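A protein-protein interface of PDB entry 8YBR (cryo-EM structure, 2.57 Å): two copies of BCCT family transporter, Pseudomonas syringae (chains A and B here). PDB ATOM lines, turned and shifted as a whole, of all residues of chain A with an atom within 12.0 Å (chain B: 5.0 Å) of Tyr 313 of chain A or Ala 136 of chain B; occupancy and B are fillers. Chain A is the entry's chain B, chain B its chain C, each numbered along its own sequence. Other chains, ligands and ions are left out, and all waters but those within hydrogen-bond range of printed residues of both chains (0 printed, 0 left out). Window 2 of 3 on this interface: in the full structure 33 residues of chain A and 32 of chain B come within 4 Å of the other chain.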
ATOM      1  N   ASN A  56     -11.312  11.335 -22.937  1.00  0.00           N
ATOM      2  CA  ASN A  56     -11.826   9.998 -23.210  1.00  0.00           C
ATOM      3  C   ASN A  56     -11.009   8.900 -22.545  1.00  0.00           C
ATOM      4  O   ASN A  56     -11.572   7.879 -22.137  1.00  0.00           O
ATOM      5  CB  ASN A  56     -11.878   9.745 -24.718  1.00  0.00           C
ATOM      6  CG  ASN A  56     -12.874  10.635 -25.426  1.00  0.00           C
ATOM      7  OD1 ASN A  56     -12.525  11.696 -25.937  1.00  0.00           O
ATOM      8  ND2 ASN A  56     -14.127  10.201 -25.466  1.00  0.00           N
ATOM      9  N   PRO A 129     -26.179  18.301 -21.151  1.00  0.00           N
ATOM     10  CA  PRO A 129     -25.516  17.048 -21.535  1.00  0.00           C
ATOM     11  C   PRO A 129     -26.483  15.940 -21.909  1.00  0.00           C
ATOM     12  O   PRO A 129     -26.051  14.948 -22.507  1.00  0.00           O
ATOM     13  CB  PRO A 129     -24.705  16.679 -20.287  1.00  0.00           C
ATOM     14  CG  PRO A 129     -25.353  17.403 -19.180  1.00  0.00           C
ATOM     15  CD  PRO A 129     -25.889  18.671 -19.759  1.00  0.00           C
ATOM     16  N   GLN A 130     -27.766  16.066 -21.576  1.00  0.00           N
ATOM     17  CA  GLN A 130     -28.765  15.069 -21.958  1.00  0.00           C
ATOM     18  C   GLN A 130     -30.147  15.687 -21.827  1.00  0.00           C
ATOM     19  O   GLN A 130     -30.520  16.140 -20.741  1.00  0.00           O
ATOM     20  CB  GLN A 130     -28.653  13.820 -21.091  1.00  0.00           C
ATOM     21  CG  GLN A 130     -28.418  14.097 -19.628  1.00  0.00           C
ATOM     22  CD  GLN A 130     -28.427  12.838 -18.798  1.00  0.00           C
ATOM     23  OE1 GLN A 130     -28.608  11.739 -19.320  1.00  0.00           O
ATOM     24  NE2 GLN A 130     -28.234  12.988 -17.496  1.00  0.00           N
ATOM     25  N   GLY A 131     -30.902  15.707 -22.915  1.00  0.00           N
ATOM     26  CA  GLY A 131     -32.249  16.239 -22.912  1.00  0.00           C
ATOM     27  C   GLY A 131     -32.393  17.398 -23.876  1.00  0.00           C
ATOM     28  O   GLY A 131     -31.498  17.706 -24.665  1.00  0.00           O
ATOM     29  N   SER A 305     -24.996   9.249  -6.313  1.00  0.00           N
ATOM     30  CA  SER A 305     -24.960   8.658  -7.644  1.00  0.00           C
ATOM     31  C   SER A 305     -24.358   9.574  -8.701  1.00  0.00           C
ATOM     32  O   SER A 305     -23.987   9.089  -9.772  1.00  0.00           O
ATOM     33  CB  SER A 305     -26.370   8.255  -8.082  1.00  0.00           C
ATOM     34  OG  SER A 305     -27.200   9.390  -8.223  1.00  0.00           O
ATOM     35  N   LYS A 306     -24.256  10.873  -8.429  1.00  0.00           N
ATOM     36  CA  LYS A 306     -23.692  11.818  -9.382  1.00  0.00           C
ATOM     37  C   LYS A 306     -22.172  11.853  -9.351  1.00  0.00           C
ATOM     38  O   LYS A 306     -21.564  12.453 -10.242  1.00  0.00           O
ATOM     39  CB  LYS A 306     -24.244  13.218  -9.110  1.00  0.00           C
ATOM     40  CG  LYS A 306     -24.287  14.116 -10.322  1.00  0.00           C
ATOM     41  CD  LYS A 306     -25.213  13.567 -11.380  1.00  0.00           C
ATOM     42  CE  LYS A 306     -25.100  14.365 -12.661  1.00  0.00           C
ATOM     43  NZ  LYS A 306     -25.915  13.780 -13.755  1.00  0.00           N
ATOM     44  N   PHE A 308     -20.184   9.382  -9.880  1.00  0.00           N
ATOM     45  CA  PHE A 308     -19.626   8.393 -10.794  1.00  0.00           C
ATOM     46  C   PHE A 308     -20.216   8.494 -12.193  1.00  0.00           C
ATOM     47  O   PHE A 308     -20.096   7.552 -12.975  1.00  0.00           O
ATOM     48  CB  PHE A 308     -19.845   6.982 -10.254  1.00  0.00           C
ATOM     49  CG  PHE A 308     -19.201   6.729  -8.927  1.00  0.00           C
ATOM     50  CD1 PHE A 308     -17.861   6.409  -8.844  1.00  0.00           C
ATOM     51  CD2 PHE A 308     -19.941   6.788  -7.763  1.00  0.00           C
ATOM     52  CE1 PHE A 308     -17.274   6.166  -7.629  1.00  0.00           C
ATOM     53  CE2 PHE A 308     -19.356   6.546  -6.546  1.00  0.00           C
ATOM     54  CZ  PHE A 308     -18.022   6.234  -6.479  1.00  0.00           C
ATOM     55  N   ASP A 309     -20.851   9.608 -12.531  1.00  0.00           N
ATOM     56  CA  ASP A 309     -21.563   9.730 -13.795  1.00  0.00           C
ATOM     57  C   ASP A 309     -20.602  10.165 -14.893  1.00  0.00           C
ATOM     58  O   ASP A 309     -20.017  11.250 -14.821  1.00  0.00           O
ATOM     59  CB  ASP A 309     -22.719  10.717 -13.670  1.00  0.00           C
ATOM     60  CG  ASP A 309     -23.882  10.361 -14.564  1.00  0.00           C
ATOM     61  OD1 ASP A 309     -23.649   9.801 -15.651  1.00  0.00           O
ATOM     62  OD2 ASP A 309     -25.034  10.633 -14.178  1.00  0.00           O
ATOM     63  N   VAL A 310     -20.448   9.318 -15.908  1.00  0.00           N
ATOM     64  CA  VAL A 310     -19.611   9.605 -17.062  1.00  0.00           C
ATOM     65  C   VAL A 310     -20.387   9.563 -18.366  1.00  0.00           C
ATOM     66  O   VAL A 310     -19.784   9.698 -19.432  1.00  0.00           O
ATOM     67  CB  VAL A 310     -18.404   8.647 -17.131  1.00  0.00           C
ATOM     68  CG1 VAL A 310     -17.377   9.010 -16.082  1.00  0.00           C
ATOM     69  CG2 VAL A 310     -18.852   7.224 -16.937  1.00  0.00           C
ATOM     70  N   TYR A 311     -21.707   9.374 -18.312  1.00  0.00           N
ATOM     71  CA  TYR A 311     -22.576   9.332 -19.490  1.00  0.00           C
ATOM     72  C   TYR A 311     -22.120   8.252 -20.471  1.00  0.00           C
ATOM     73  O   TYR A 311     -21.848   8.508 -21.642  1.00  0.00           O
ATOM     74  CB  TYR A 311     -22.644  10.706 -20.164  1.00  0.00           C
ATOM     75  CG  TYR A 311     -22.911  11.832 -19.195  1.00  0.00           C
ATOM     76  CD1 TYR A 311     -24.200  12.139 -18.803  1.00  0.00           C
ATOM     77  CD2 TYR A 311     -21.873  12.578 -18.666  1.00  0.00           C
ATOM     78  CE1 TYR A 311     -24.446  13.152 -17.915  1.00  0.00           C
ATOM     79  CE2 TYR A 311     -22.112  13.591 -17.777  1.00  0.00           C
ATOM     80  CZ  TYR A 311     -23.399  13.873 -17.405  1.00  0.00           C
ATOM     81  OH  TYR A 311     -23.644  14.888 -16.517  1.00  0.00           O
ATOM     82  N   ALA A 312     -22.058   7.022 -19.966  1.00  0.00           N
ATOM     83  CA  ALA A 312     -21.459   5.920 -20.705  1.00  0.00           C
ATOM     84  C   ALA A 312     -22.415   5.245 -21.677  1.00  0.00           C
ATOM     85  O   ALA A 312     -21.957   4.492 -22.539  1.00  0.00           O
ATOM     86  CB  ALA A 312     -20.910   4.879 -19.734  1.00  0.00           C
ATOM     87  N   TYR A 313     -23.718   5.487 -21.566  1.00  0.00           N
ATOM     88  CA  TYR A 313     -24.695   4.860 -22.445  1.00  0.00           C
ATOM     89  C   TYR A 313     -25.264   5.831 -23.471  1.00  0.00           C
ATOM     90  O   TYR A 313     -26.194   5.474 -24.196  1.00  0.00           O
ATOM     91  CB  TYR A 313     -25.823   4.237 -21.622  1.00  0.00           C
ATOM     92  CG  TYR A 313     -25.397   3.020 -20.832  1.00  0.00           C
ATOM     93  CD1 TYR A 313     -25.177   1.807 -21.457  1.00  0.00           C
ATOM     94  CD2 TYR A 313     -25.213   3.087 -19.460  1.00  0.00           C
ATOM     95  CE1 TYR A 313     -24.784   0.700 -20.743  1.00  0.00           C
ATOM     96  CE2 TYR A 313     -24.819   1.983 -18.740  1.00  0.00           C
ATOM     97  CZ  TYR A 313     -24.609   0.794 -19.386  1.00  0.00           C
ATOM     98  OH  TYR A 313     -24.221  -0.310 -18.670  1.00  0.00           O
ATOM     99  N   ASN A 314     -24.729   7.043 -23.548  1.00  0.00           N
ATOM    100  CA  ASN A 314     -25.135   8.030 -24.535  1.00  0.00           C
ATOM    101  C   ASN A 314     -24.187   8.011 -25.727  1.00  0.00           C
ATOM    102  O   ASN A 314     -23.160   7.332 -25.729  1.00  0.00           O
ATOM    103  CB  ASN A 314     -25.170   9.427 -23.916  1.00  0.00           C
ATOM    104  CG  ASN A 314     -26.182   9.545 -22.808  1.00  0.00           C
ATOM    105  OD1 ASN A 314     -27.141   8.779 -22.745  1.00  0.00           O
ATOM    106  ND2 ASN A 314     -25.985  10.515 -21.930  1.00  0.00           N
ATOM    107  N   LYS A 315     -24.549   8.773 -26.750  1.00  0.00           N
ATOM    108  CA  LYS A 315     -23.690   8.895 -27.917  1.00  0.00           C
ATOM    109  C   LYS A 315     -22.406   9.624 -27.527  1.00  0.00           C
ATOM    110  O   LYS A 315     -22.450  10.566 -26.730  1.00  0.00           O
ATOM    111  CB  LYS A 315     -24.413   9.647 -29.034  1.00  0.00           C
ATOM    112  CG  LYS A 315     -25.599   8.907 -29.628  1.00  0.00           C
ATOM    113  CD  LYS A 315     -26.291   9.710 -30.713  1.00  0.00           C
ATOM    114  CE  LYS A 315     -27.457   8.933 -31.302  1.00  0.00           C
ATOM    115  NZ  LYS A 315     -28.166   9.711 -32.353  1.00  0.00           N
ATOM    116  N   PRO A 316     -21.251   9.196 -28.037  1.00  0.00           N
ATOM    117  CA  PRO A 316     -19.987   9.831 -27.641  1.00  0.00           C
ATOM    118  C   PRO A 316     -19.972  11.326 -27.919  1.00  0.00           C
ATOM    119  O   PRO A 316     -20.621  11.819 -28.842  1.00  0.00           O
ATOM    120  CB  PRO A 316     -18.946   9.098 -28.488  1.00  0.00           C
ATOM    121  CG  PRO A 316     -19.541   7.768 -28.725  1.00  0.00           C
ATOM    122  CD  PRO A 316     -21.024   7.971 -28.822  1.00  0.00           C
ATOM    123  N   SER A 317     -19.208  12.045 -27.106  1.00  0.00           N
ATOM    124  CA  SER A 317     -19.170  13.502 -27.160  1.00  0.00           C
ATOM    125  C   SER A 317     -17.918  13.970 -26.429  1.00  0.00           C
ATOM    126  O   SER A 317     -17.107  13.164 -25.966  1.00  0.00           O
ATOM    127  CB  SER A 317     -20.439  14.104 -26.558  1.00  0.00           C
ATOM    128  OG  SER A 317     -20.181  15.362 -25.975  1.00  0.00           O
ATOM    129  N   LEU A 320     -17.422  15.970 -21.285  1.00  0.00           N
ATOM    130  CA  LEU A 320     -16.835  15.679 -19.981  1.00  0.00           C
ATOM    131  C   LEU A 320     -15.461  16.311 -19.815  1.00  0.00           C
ATOM    132  O   LEU A 320     -15.069  16.643 -18.694  1.00  0.00           O
ATOM    133  CB  LEU A 320     -16.751  14.168 -19.779  1.00  0.00           C
ATOM    134  CG  LEU A 320     -16.674  13.653 -18.343  1.00  0.00           C
ATOM    135  CD1 LEU A 320     -18.024  13.721 -17.670  1.00  0.00           C
ATOM    136  CD2 LEU A 320     -16.144  12.239 -18.324  1.00  0.00           C
ATOM    137  N   GLY B 134     -34.932  -2.899 -25.777  1.00  0.00           N
ATOM    138  CA  GLY B 134     -34.111  -2.647 -26.937  1.00  0.00           C
ATOM    139  C   GLY B 134     -33.473  -1.279 -26.963  1.00  0.00           C
ATOM    140  O   GLY B 134     -32.763  -0.967 -27.924  1.00  0.00           O
ATOM    141  N   THR B 135     -33.700  -0.461 -25.942  1.00  0.00           N
ATOM    142  CA  THR B 135     -33.219   0.907 -25.895  1.00  0.00           C
ATOM    143  C   THR B 135     -31.954   0.988 -25.048  1.00  0.00           C
ATOM    144  O   THR B 135     -31.403  -0.024 -24.613  1.00  0.00           O
ATOM    145  CB  THR B 135     -34.310   1.830 -25.347  1.00  0.00           C
ATOM    146  OG1 THR B 135     -34.687   1.401 -24.035  1.00  0.00           O
ATOM    147  CG2 THR B 135     -35.530   1.805 -26.240  1.00  0.00           C
ATOM    148  N   ALA B 136     -31.481   2.209 -24.814  1.00  0.00           N
ATOM    149  CA  ALA B 136     -30.346   2.457 -23.937  1.00  0.00           C
ATOM    150  C   ALA B 136     -30.767   2.748 -22.504  1.00  0.00           C
ATOM    151  O   ALA B 136     -29.902   2.901 -21.639  1.00  0.00           O
ATOM    152  CB  ALA B 136     -29.509   3.619 -24.471  1.00  0.00           C
ATOM    153  N   GLU B 137     -32.066   2.845 -22.238  1.00  0.00           N
ATOM    154  CA  GLU B 137     -32.555   2.870 -20.867  1.00  0.00           C
ATOM    155  C   GLU B 137     -32.762   1.471 -20.316  1.00  0.00           C
ATOM    156  O   GLU B 137     -32.502   1.230 -19.133  1.00  0.00           O
ATOM    157  CB  GLU B 137     -33.862   3.659 -20.779  1.00  0.00           C
ATOM    158  CG  GLU B 137     -33.674   5.158 -20.632  1.00  0.00           C
ATOM    159  CD  GLU B 137     -33.391   5.860 -21.947  1.00  0.00           C
ATOM    160  OE1 GLU B 137     -33.555   7.096 -22.002  1.00  0.00           O
ATOM    161  OE2 GLU B 137     -33.026   5.185 -22.932  1.00  0.00           O
ATOM    162  N   ALA B 138     -33.202   0.539 -21.159  1.00  0.00           N
ATOM    163  CA  ALA B 138     -33.303  -0.850 -20.736  1.00  0.00           C
ATOM    164  C   ALA B 138     -31.930  -1.436 -20.447  1.00  0.00           C
ATOM    165  O   ALA B 138     -31.775  -2.242 -19.525  1.00  0.00           O
ATOM    166  CB  ALA B 138     -34.027  -1.669 -21.800  1.00  0.00           C
ATOM    167  N   ALA B 139     -30.915  -1.035 -21.215  1.00  0.00           N
ATOM    168  CA  ALA B 139     -29.563  -1.527 -20.976  1.00  0.00           C
ATOM    169  C   ALA B 139     -29.000  -1.014 -19.661  1.00  0.00           C
ATOM    170  O   ALA B 139     -28.226  -1.717 -19.004  1.00  0.00           O
ATOM    171  CB  ALA B 139     -28.645  -1.127 -22.129  1.00  0.00           C
ATOM    172  N   ARG B 140     -29.364   0.199 -19.264  1.00  0.00           N
ATOM    173  CA  ARG B 140     -28.902   0.740 -17.996  1.00  0.00           C
ATOM    174  C   ARG B 140     -29.707   0.204 -16.823  1.00  0.00           C
ATOM    175  O   ARG B 140     -29.183   0.106 -15.711  1.00  0.00           O
ATOM    176  CB  ARG B 140     -28.970   2.263 -18.034  1.00  0.00           C
ATOM    177  CG  ARG B 140     -28.232   2.955 -16.917  1.00  0.00           C
ATOM    178  CD  ARG B 140     -28.448   4.448 -16.986  1.00  0.00           C
ATOM    179  NE  ARG B 140     -27.776   5.142 -15.897  1.00  0.00           N
ATOM    180  CZ  ARG B 140     -27.877   6.447 -15.674  1.00  0.00           C
ATOM    181  NH1 ARG B 140     -28.626   7.199 -16.463  1.00  0.00           N
ATOM    182  NH2 ARG B 140     -27.232   6.996 -14.657  1.00  0.00           N
ATOM    183  N   MET B 143     -28.668  -3.684 -15.974  1.00  0.00           N
ATOM    184  CA  MET B 143     -27.371  -3.884 -15.347  1.00  0.00           C
ATOM    185  C   MET B 143     -27.376  -3.531 -13.869  1.00  0.00           C
ATOM    186  O   MET B 143     -26.381  -3.785 -13.189  1.00  0.00           O
ATOM    187  CB  MET B 143     -26.297  -3.062 -16.062  1.00  0.00           C
ATOM    188  CG  MET B 143     -25.902  -3.582 -17.436  1.00  0.00           C
ATOM    189  SD  MET B 143     -25.248  -5.262 -17.465  1.00  0.00           S
ATOM    190  CE  MET B 143     -23.875  -5.128 -16.336  1.00  0.00           C
ATOM    191  N   THR B 291     -17.934   1.935 -18.451  1.00  0.00           N
ATOM    192  CA  THR B 291     -19.180   1.372 -17.939  1.00  0.00           C
ATOM    193  C   THR B 291     -18.987   0.697 -16.586  1.00  0.00           C
ATOM    194  O   THR B 291     -19.927   0.651 -15.783  1.00  0.00           O
ATOM    195  CB  THR B 291     -19.777   0.393 -18.943  1.00  0.00           C
ATOM    196  OG1 THR B 291     -18.752  -0.471 -19.434  1.00  0.00           O
ATOM    197  CG2 THR B 291     -20.388   1.138 -20.104  1.00  0.00           C
ATOM    198  N   GLN B 294     -19.524   3.485 -14.249  1.00  0.00           N
ATOM    199  CA  GLN B 294     -20.926   3.900 -14.250  1.00  0.00           C
ATOM    200  C   GLN B 294     -21.796   2.971 -13.400  1.00  0.00           C
ATOM    201  O   GLN B 294     -22.674   3.432 -12.652  1.00  0.00           O
ATOM    202  CB  GLN B 294     -21.443   3.944 -15.685  1.00  0.00           C
ATOM    203  CG  GLN B 294     -22.888   4.352 -15.822  1.00  0.00           C
ATOM    204  CD  GLN B 294     -23.045   5.830 -16.051  1.00  0.00           C
ATOM    205  OE1 GLN B 294     -22.067   6.550 -16.184  1.00  0.00           O
ATOM    206  NE2 GLN B 294     -24.280   6.291 -16.099  1.00  0.00           N
ATOM    207  N   ASN B 295     -21.568   1.659 -13.509  1.00  0.00           N
ATOM    208  CA  ASN B 295     -22.427   0.686 -12.838  1.00  0.00           C
ATOM    209  C   ASN B 295     -22.337   0.791 -11.320  1.00  0.00           C
ATOM    210  O   ASN B 295     -23.340   0.611 -10.620  1.00  0.00           O
ATOM    211  CB  ASN B 295     -22.066  -0.726 -13.293  1.00  0.00           C
ATOM    212  CG  ASN B 295     -22.493  -1.010 -14.714  1.00  0.00           C
ATOM    213  OD1 ASN B 295     -23.457  -0.441 -15.211  1.00  0.00           O
ATOM    214  ND2 ASN B 295     -21.776  -1.902 -15.373  1.00  0.00           N
ATOM    215  N   ASN B 375     -21.444  -6.235 -20.113  1.00  0.00           N
ATOM    216  CA  ASN B 375     -21.355  -5.111 -21.033  1.00  0.00           C
ATOM    217  C   ASN B 375     -20.706  -5.511 -22.349  1.00  0.00           C
ATOM    218  O   ASN B 375     -21.050  -4.952 -23.396  1.00  0.00           O
ATOM    219  CB  ASN B 375     -20.596  -3.961 -20.386  1.00  0.00           C
ATOM    220  CG  ASN B 375     -21.455  -3.167 -19.437  1.00  0.00           C
ATOM    221  OD1 ASN B 375     -22.363  -2.455 -19.853  1.00  0.00           O
ATOM    222  ND2 ASN B 375     -21.172  -3.278 -18.153  1.00  0.00           N
ATOM    223  N   LEU B 382     -26.534  -4.131 -29.069  1.00  0.00           N
ATOM    224  CA  LEU B 382     -27.033  -2.807 -29.440  1.00  0.00           C
ATOM    225  C   LEU B 382     -26.299  -2.227 -30.642  1.00  0.00           C
ATOM    226  O   LEU B 382     -26.927  -1.831 -31.628  1.00  0.00           O
ATOM    227  CB  LEU B 382     -26.928  -1.829 -28.271  1.00  0.00           C
ATOM    228  CG  LEU B 382     -27.908  -1.916 -27.109  1.00  0.00           C
ATOM    229  CD1 LEU B 382     -27.526  -0.896 -26.061  1.00  0.00           C
ATOM    230  CD2 LEU B 382     -29.312  -1.669 -27.602  1.00  0.00           C
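The side-chain carboxylate of Asp 309 of chain A lies within salt-bridge range of the side-chain amino group of Lys 306 of chain A, 3.3 Å away. OD1 of Asp 309 of chain A lies within hydrogen-bond range of N of Tyr 311 of chain A, 3.3 Å away. The guanidinium group (NH2) of Arg 140 of chain B lies close to the side-chain amide nitrogen (NE2) of Gln 294 of chain B, at 3.4 Å. The backbone carbonyl oxygen (O) of Thr 291 of chain B lies within hydrogen-bond range of the side-chain amide nitrogen (ND2) of Asn 295 of chain B (3.2 Å). ND2 of Asn 375 of chain B lies close to ND2 of Asn 295 of chain B, 3.2 Å away.
Of the printed residues of chain B, Tyr 313 of chain A touches Ala 136, Arg 140, Met 143, Asn 295 and Asn 375. Of chain A, only Tyr 313 comes within 4 Å of Ala 136 of chain B. No residue of chain A comes within 4 Å of Gly 134 of chain B. No residue of chain A comes within 4 Å of Thr 135 of chain B. No residue of chain A comes within 4 Å of Glu 137 of chain B. No residue of chain A comes within 4 Å of Ala 138 of chain B. Printed residues of chain A within 4 Å of Arg 140 of chain B: Tyr 313 (3.9 Å). Of chain A, only Tyr 313 comes within 4 Å of Met 143 of chain B. Printed residues of chain B within 4 Å of Val 310 of chain A: Gln 294 (3.2 Å). Of the printed residues of chain A, Asn 295 of chain B touches Tyr 313 (3.5 Å). Of the printed residues of chain B, Tyr 311 of chain A touches Gln 294 (3.6 Å). Ser 317 of chain A touches none of the printed residues of chain B. Pro 316 of chain A touches none of the printed residues of chain B. The nearest printed residue of chain B that does not touch Asp 309 of chain A is Arg 140 of chain B (4.3 Å).
Of the 17 printed residues of chain A, 6 touch a printed residue of chain B. Hydrophobic or aromatic side chains of chain A within 4 Å of the printed part of chain B: Val 310, Ala 312 and Tyr 313. Of the 13 printed residues of chain B, 7 touch a printed residue of chain A. Among the printed residues, no Asp or Glu carboxylate lies within 4 Å of a Lys or Arg side-chain nitrogen of the other chain.
Among the printed residues, merely in contact across the chains: Tyr 313 of chain A with Asn 295 of chain B (3.5 Å), Tyr 311 of chain A with Gln 294 of chain B (3.6 Å), Asp 309 of chain A with Gln 294 of chain B (3.6 Å), Ala 312 of chain A with Thr 291 of chain B (3.8 Å), Tyr 313 of chain A with Ala 136 of chain B (3.8 Å), Ala 312 of chain A with Gln 294 of chain B (3.8 Å), Tyr 313 of chain A with Met 143 of chain B (3.9 Å), Phe 308 of chain A with Gln 294 of chain B (3.9 Å) and Tyr 313 of chain A with Arg 140 of chain B (3.9 Å).
No position is printed for both chains. Of the 11 pairs that touch across the chains among the printed residues, none has its exchanged pair printed and touching as well.
The side-chain amide oxygen (OE1) of Gln 294 of chain B sits at hydrogen-bond distance from the backbone NH (N) of Val 310 of chain A. The side-chain hydroxyl of Tyr 313 of chain A is in hydrogen-bond range of the side-chain amide oxygen of Asn 375 of chain B, at 3.1 Å.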
